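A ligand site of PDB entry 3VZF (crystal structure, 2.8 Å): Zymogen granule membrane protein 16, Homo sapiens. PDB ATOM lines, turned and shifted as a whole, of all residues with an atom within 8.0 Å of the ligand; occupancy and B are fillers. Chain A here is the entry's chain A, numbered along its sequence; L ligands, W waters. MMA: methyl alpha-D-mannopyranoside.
The side-chain carboxylate of Asp 133 sits at hydrogen-bond distance from an oxygen (O4) of the ligand, 2.7 Å away.
The backbone NH of Leu 131 lies within hydrogen-bond range of an oxygen (O6) of the ligand, at 2.9 Å.
O of Leu 131 lies within hydrogen-bond range of O6 of the ligand.
O5 of the ligand lies within hydrogen-bond range of N of Ser 130 (3.0 Å).
An oxygen (O5) of the ligand is in hydrogen-bond range of the side-chain hydroxyl (OG) of Ser 130 (3.0 Å).
An oxygen (O3) of the ligand sits at hydrogen-bond distance from the backbone NH of Gly 17 (3.0 Å).
N of Gly 129 sits at hydrogen-bond distance from O6 of the ligand (3.1 Å).
The backbone NH (N) of Gly 129 lies within hydrogen-bond range of the side-chain carboxylate (OD2) of Asp 133, 3.3 Å away.
The backbone carbonyl oxygen (O) of Arg 127 lies within hydrogen-bond range of the backbone NH (N) of Asp 133 (3.0 Å).
The backbone carbonyl oxygen (O) of Asp 133 is in hydrogen-bond range of the backbone NH (N) of Ser 14.
O of Ser 130 lies close to N of Gly 60 (3.2 Å).
The guanidinium group of Arg 127 sits at hydrogen-bond distance from the backbone carbonyl oxygen of Gly 17 (3.0 Å).
CE1 of Tyr 86 touches O4 of the ligand, 3.4 Å away.
Hydrophobic or aromatic side chains within 4 Å of the ligand: Tyr 86 and Leu 131.
The nearest printed residue that does not touch the ligand is Gly 16 (4.02 Å).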
ATOM      1  N   SER A  14       1.710 -10.540  -3.694  1.00  0.00           N
ATOM      2  CA  SER A  14       0.448 -10.397  -4.433  1.00  0.00           C
ATOM      3  C   SER A  14      -0.772 -10.796  -3.595  1.00  0.00           C
ATOM      4  O   SER A  14      -0.644 -11.147  -2.421  1.00  0.00           O
ATOM      5  CB  SER A  14       0.494 -11.189  -5.745  1.00  0.00           C
ATOM      6  OG  SER A  14      -0.459 -10.693  -6.669  1.00  0.00           O
ATOM      7  N   GLY A  15      -1.953 -10.719  -4.208  1.00  0.00           N
ATOM      8  CA  GLY A  15      -3.219 -10.926  -3.490  1.00  0.00           C
ATOM      9  C   GLY A  15      -3.843 -12.293  -3.660  1.00  0.00           C
ATOM     10  O   GLY A  15      -5.058 -12.408  -3.851  1.00  0.00           O
ATOM     11  N   GLY A  16      -3.021 -13.340  -3.575  1.00  0.00           N
ATOM     12  CA  GLY A  16      -3.488 -14.720  -3.641  1.00  0.00           C
ATOM     13  C   GLY A  16      -3.579 -15.353  -2.270  1.00  0.00           C
ATOM     14  O   GLY A  16      -2.980 -14.868  -1.313  1.00  0.00           O
ATOM     15  N   GLY A  17      -4.336 -16.438  -2.174  1.00  0.00           N
ATOM     16  CA  GLY A  17      -4.504 -17.159  -0.906  1.00  0.00           C
ATOM     17  C   GLY A  17      -5.297 -16.393   0.141  1.00  0.00           C
ATOM     18  O   GLY A  17      -5.892 -15.361  -0.162  1.00  0.00           O
ATOM     19  N   LYS A  18      -5.288 -16.905   1.368  1.00  0.00           N
ATOM     20  CA  LYS A  18      -5.988 -16.277   2.482  1.00  0.00           C
ATOM     21  C   LYS A  18      -5.046 -15.442   3.340  1.00  0.00           C
ATOM     22  O   LYS A  18      -3.826 -15.651   3.318  1.00  0.00           O
ATOM     23  CB  LYS A  18      -6.724 -17.329   3.321  1.00  0.00           C
ATOM     24  CG  LYS A  18      -8.014 -17.837   2.679  1.00  0.00           C
ATOM     25  CD  LYS A  18      -9.190 -16.900   2.980  1.00  0.00           C
ATOM     26  CE  LYS A  18     -10.255 -16.970   1.894  1.00  0.00           C
ATOM     27  NZ  LYS A  18      -9.836 -16.265   0.641  1.00  0.00           N
ATOM     28  N   TYR A  42      10.739 -20.445  -4.084  1.00  0.00           N
ATOM     29  CA  TYR A  42       9.840 -19.663  -3.229  1.00  0.00           C
ATOM     30  C   TYR A  42      10.075 -19.794  -1.724  1.00  0.00           C
ATOM     31  O   TYR A  42      10.842 -20.641  -1.262  1.00  0.00           O
ATOM     32  CB  TYR A  42       8.382 -20.000  -3.541  1.00  0.00           C
ATOM     33  CG  TYR A  42       7.998 -19.855  -4.991  1.00  0.00           C
ATOM     34  CD1 TYR A  42       7.949 -18.612  -5.598  1.00  0.00           C
ATOM     35  CD2 TYR A  42       7.679 -20.976  -5.754  1.00  0.00           C
ATOM     36  CE1 TYR A  42       7.596 -18.474  -6.940  1.00  0.00           C
ATOM     37  CE2 TYR A  42       7.318 -20.859  -7.099  1.00  0.00           C
ATOM     38  CZ  TYR A  42       7.280 -19.609  -7.676  1.00  0.00           C
ATOM     39  OH  TYR A  42       6.933 -19.479  -9.005  1.00  0.00           O
ATOM     40  N   ILE A  43       9.396 -18.935  -0.971  1.00  0.00           N
ATOM     41  CA  ILE A  43       9.250 -19.097   0.467  1.00  0.00           C
ATOM     42  C   ILE A  43       7.894 -19.738   0.728  1.00  0.00           C
ATOM     43  O   ILE A  43       6.842 -19.156   0.438  1.00  0.00           O
ATOM     44  CB  ILE A  43       9.481 -17.778   1.236  1.00  0.00           C
ATOM     45  CG1 ILE A  43      10.987 -17.549   1.404  1.00  0.00           C
ATOM     46  CG2 ILE A  43       8.793 -17.805   2.596  1.00  0.00           C
ATOM     47  CD1 ILE A  43      11.370 -16.232   2.029  1.00  0.00           C
ATOM     48  N   VAL A  44       7.949 -20.959   1.251  1.00  0.00           N
ATOM     49  CA  VAL A  44       6.788 -21.835   1.343  1.00  0.00           C
ATOM     50  C   VAL A  44       6.000 -21.547   2.615  1.00  0.00           C
ATOM     51  O   VAL A  44       4.781 -21.407   2.578  1.00  0.00           O
ATOM     52  CB  VAL A  44       7.219 -23.329   1.309  1.00  0.00           C
ATOM     53  CG1 VAL A  44       6.025 -24.234   1.169  1.00  0.00           C
ATOM     54  CG2 VAL A  44       8.189 -23.585   0.166  1.00  0.00           C
ATOM     55  N   GLY A  59       1.324 -21.387   5.494  1.00  0.00           N
ATOM     56  CA  GLY A  59       1.970 -21.741   4.230  1.00  0.00           C
ATOM     57  C   GLY A  59       1.798 -23.203   3.872  1.00  0.00           C
ATOM     58  O   GLY A  59       0.817 -23.841   4.274  1.00  0.00           O
ATOM     59  N   GLY A  60       2.744 -23.747   3.121  1.00  0.00           N
ATOM     60  CA  GLY A  60       2.665 -25.132   2.645  1.00  0.00           C
ATOM     61  C   GLY A  60       3.750 -26.060   3.175  1.00  0.00           C
ATOM     62  O   GLY A  60       4.559 -25.669   4.019  1.00  0.00           O
ATOM     63  N   TRP A  85       4.846 -13.140  -7.814  1.00  0.00           N
ATOM     64  CA  TRP A  85       3.461 -13.244  -7.373  1.00  0.00           C
ATOM     65  C   TRP A  85       3.488 -13.806  -5.958  1.00  0.00           C
ATOM     66  O   TRP A  85       2.534 -13.654  -5.193  1.00  0.00           O
ATOM     67  CB  TRP A  85       2.664 -14.162  -8.293  1.00  0.00           C
ATOM     68  CG  TRP A  85       2.695 -13.737  -9.736  1.00  0.00           C
ATOM     69  CD1 TRP A  85       3.619 -14.071 -10.679  1.00  0.00           C
ATOM     70  CD2 TRP A  85       1.746 -12.876 -10.386  1.00  0.00           C
ATOM     71  NE1 TRP A  85       3.313 -13.485 -11.876  1.00  0.00           N
ATOM     72  CE2 TRP A  85       2.172 -12.746 -11.729  1.00  0.00           C
ATOM     73  CE3 TRP A  85       0.586 -12.213  -9.977  1.00  0.00           C
ATOM     74  CZ2 TRP A  85       1.475 -11.968 -12.659  1.00  0.00           C
ATOM     75  CZ3 TRP A  85      -0.115 -11.444 -10.904  1.00  0.00           C
ATOM     76  CH2 TRP A  85       0.336 -11.330 -12.231  1.00  0.00           C
ATOM     77  N   TYR A  86       4.605 -14.466  -5.622  1.00  0.00           N
ATOM     78  CA  TYR A  86       4.822 -15.091  -4.321  1.00  0.00           C
ATOM     79  C   TYR A  86       6.158 -14.645  -3.734  1.00  0.00           C
ATOM     80  O   TYR A  86       7.111 -14.365  -4.474  1.00  0.00           O
ATOM     81  CB  TYR A  86       4.809 -16.618  -4.440  1.00  0.00           C
ATOM     82  CG  TYR A  86       3.634 -17.165  -5.211  1.00  0.00           C
ATOM     83  CD1 TYR A  86       2.348 -17.125  -4.677  1.00  0.00           C
ATOM     84  CD2 TYR A  86       3.808 -17.746  -6.467  1.00  0.00           C
ATOM     85  CE1 TYR A  86       1.267 -17.634  -5.370  1.00  0.00           C
ATOM     86  CE2 TYR A  86       2.729 -18.253  -7.182  1.00  0.00           C
ATOM     87  CZ  TYR A  86       1.457 -18.198  -6.623  1.00  0.00           C
ATOM     88  OH  TYR A  86       0.363 -18.705  -7.294  1.00  0.00           O
ATOM     89  N   ARG A 127      -0.359 -12.852   3.438  1.00  0.00           N
ATOM     90  CA  ARG A 127      -1.270 -13.828   2.842  1.00  0.00           C
ATOM     91  C   ARG A 127      -0.506 -15.101   2.511  1.00  0.00           C
ATOM     92  O   ARG A 127       0.672 -15.053   2.121  1.00  0.00           O
ATOM     93  CB  ARG A 127      -1.912 -13.269   1.573  1.00  0.00           C
ATOM     94  CG  ARG A 127      -2.649 -11.952   1.781  1.00  0.00           C
ATOM     95  CD  ARG A 127      -3.327 -11.464   0.497  1.00  0.00           C
ATOM     96  NE  ARG A 127      -4.586 -12.172   0.235  1.00  0.00           N
ATOM     97  CZ  ARG A 127      -5.750 -11.903   0.840  1.00  0.00           C
ATOM     98  NH1 ARG A 127      -5.829 -10.948   1.765  1.00  0.00           N
ATOM     99  NH2 ARG A 127      -6.829 -12.602   0.524  1.00  0.00           N
ATOM    100  N   SER A 128      -1.172 -16.239   2.686  1.00  0.00           N
ATOM    101  CA  SER A 128      -0.559 -17.535   2.402  1.00  0.00           C
ATOM    102  C   SER A 128      -1.555 -18.576   1.876  1.00  0.00           C
ATOM    103  O   SER A 128      -2.772 -18.437   2.051  1.00  0.00           O
ATOM    104  CB  SER A 128       0.169 -18.073   3.638  1.00  0.00           C
ATOM    105  OG  SER A 128      -0.750 -18.483   4.647  1.00  0.00           O
ATOM    106  N   GLY A 129      -1.009 -19.594   1.229  1.00  0.00           N
ATOM    107  CA  GLY A 129      -1.763 -20.768   0.793  1.00  0.00           C
ATOM    108  C   GLY A 129      -0.821 -21.951   0.890  1.00  0.00           C
ATOM    109  O   GLY A 129      -0.493 -22.388   1.990  1.00  0.00           O
ATOM    110  N   SER A 130      -0.393 -22.457  -0.256  1.00  0.00           N
ATOM    111  CA  SER A 130       0.623 -23.504  -0.297  1.00  0.00           C
ATOM    112  C   SER A 130       2.022 -22.884  -0.297  1.00  0.00           C
ATOM    113  O   SER A 130       3.019 -23.579  -0.091  1.00  0.00           O
ATOM    114  CB  SER A 130       0.424 -24.415  -1.523  1.00  0.00           C
ATOM    115  OG  SER A 130       0.707 -23.716  -2.725  1.00  0.00           O
ATOM    116  N   LEU A 131       2.062 -21.573  -0.538  1.00  0.00           N
ATOM    117  CA  LEU A 131       3.279 -20.757  -0.430  1.00  0.00           C
ATOM    118  C   LEU A 131       2.976 -19.484   0.370  1.00  0.00           C
ATOM    119  O   LEU A 131       1.855 -19.301   0.855  1.00  0.00           O
ATOM    120  CB  LEU A 131       3.802 -20.378  -1.825  1.00  0.00           C
ATOM    121  CG  LEU A 131       4.294 -21.492  -2.754  1.00  0.00           C
ATOM    122  CD1 LEU A 131       4.493 -20.951  -4.160  1.00  0.00           C
ATOM    123  CD2 LEU A 131       5.580 -22.140  -2.238  1.00  0.00           C
ATOM    124  N   ILE A 132       3.978 -18.627   0.536  1.00  0.00           N
ATOM    125  CA  ILE A 132       3.745 -17.306   1.113  1.00  0.00           C
ATOM    126  C   ILE A 132       3.523 -16.304  -0.015  1.00  0.00           C
ATOM    127  O   ILE A 132       4.471 -15.913  -0.710  1.00  0.00           O
ATOM    128  CB  ILE A 132       4.869 -16.845   2.088  1.00  0.00           C
ATOM    129  CG1 ILE A 132       5.020 -17.822   3.263  1.00  0.00           C
ATOM    130  CG2 ILE A 132       4.602 -15.428   2.610  1.00  0.00           C
ATOM    131  CD1 ILE A 132       3.817 -17.891   4.205  1.00  0.00           C
ATOM    132  N   ASP A 133       2.269 -15.922  -0.203  1.00  0.00           N
ATOM    133  CA  ASP A 133       1.888 -14.987  -1.257  1.00  0.00           C
ATOM    134  C   ASP A 133       2.406 -13.585  -0.956  1.00  0.00           C
ATOM    135  O   ASP A 133       3.012 -12.943  -1.811  1.00  0.00           O
ATOM    136  CB  ASP A 133       0.367 -14.963  -1.409  1.00  0.00           C
ATOM    137  CG  ASP A 133      -0.201 -16.302  -1.837  1.00  0.00           C
ATOM    138  OD1 ASP A 133      -0.606 -16.431  -3.006  1.00  0.00           O
ATOM    139  OD2 ASP A 133      -0.228 -17.232  -1.000  1.00  0.00           O
ATOM    140  N   ALA A 134       2.177 -13.129   0.273  1.00  0.00           N
ATOM    141  CA  ALA A 134       2.509 -11.773   0.673  1.00  0.00           C
ATOM    142  C   ALA A 134       2.918 -11.703   2.140  1.00  0.00           C
ATOM    143  O   ALA A 134       2.504 -12.533   2.948  1.00  0.00           O
ATOM    144  CB  ALA A 134       1.332 -10.857   0.407  1.00  0.00           C
HETATM  145  C1  MMA L   1      -2.720 -22.356  -3.517  1.00  0.00           C
HETATM  146  C2  MMA L   1      -3.886 -21.389  -3.335  1.00  0.00           C
HETATM  147  C3  MMA L   1      -3.572 -20.042  -3.973  1.00  0.00           C
HETATM  148  C4  MMA L   1      -2.213 -19.506  -3.515  1.00  0.00           C
HETATM  149  C5  MMA L   1      -1.122 -20.577  -3.657  1.00  0.00           C
HETATM  150  C6  MMA L   1       0.208 -20.096  -3.104  1.00  0.00           C
HETATM  151  C7  MMA L   1      -2.115 -23.965  -5.146  1.00  0.00           C
HETATM  152  O1  MMA L   1      -2.533 -22.621  -4.920  1.00  0.00           O
HETATM  153  O2  MMA L   1      -4.134 -21.202  -1.933  1.00  0.00           O
HETATM  154  O3  MMA L   1      -4.598 -19.097  -3.640  1.00  0.00           O
HETATM  155  O4  MMA L   1      -1.867 -18.367  -4.304  1.00  0.00           O
HETATM  156  O5  MMA L   1      -1.525 -21.778  -2.971  1.00  0.00           O
HETATM  157  O6  MMA L   1       0.090 -19.847  -1.698  1.00  0.00           O
HETATM  158  O   HOH W   1      -6.276 -20.081  -0.857  1.00  0.00           O
HETATM  159  O   HOH W   2      -4.893 -22.883   0.485  1.00  0.00           O
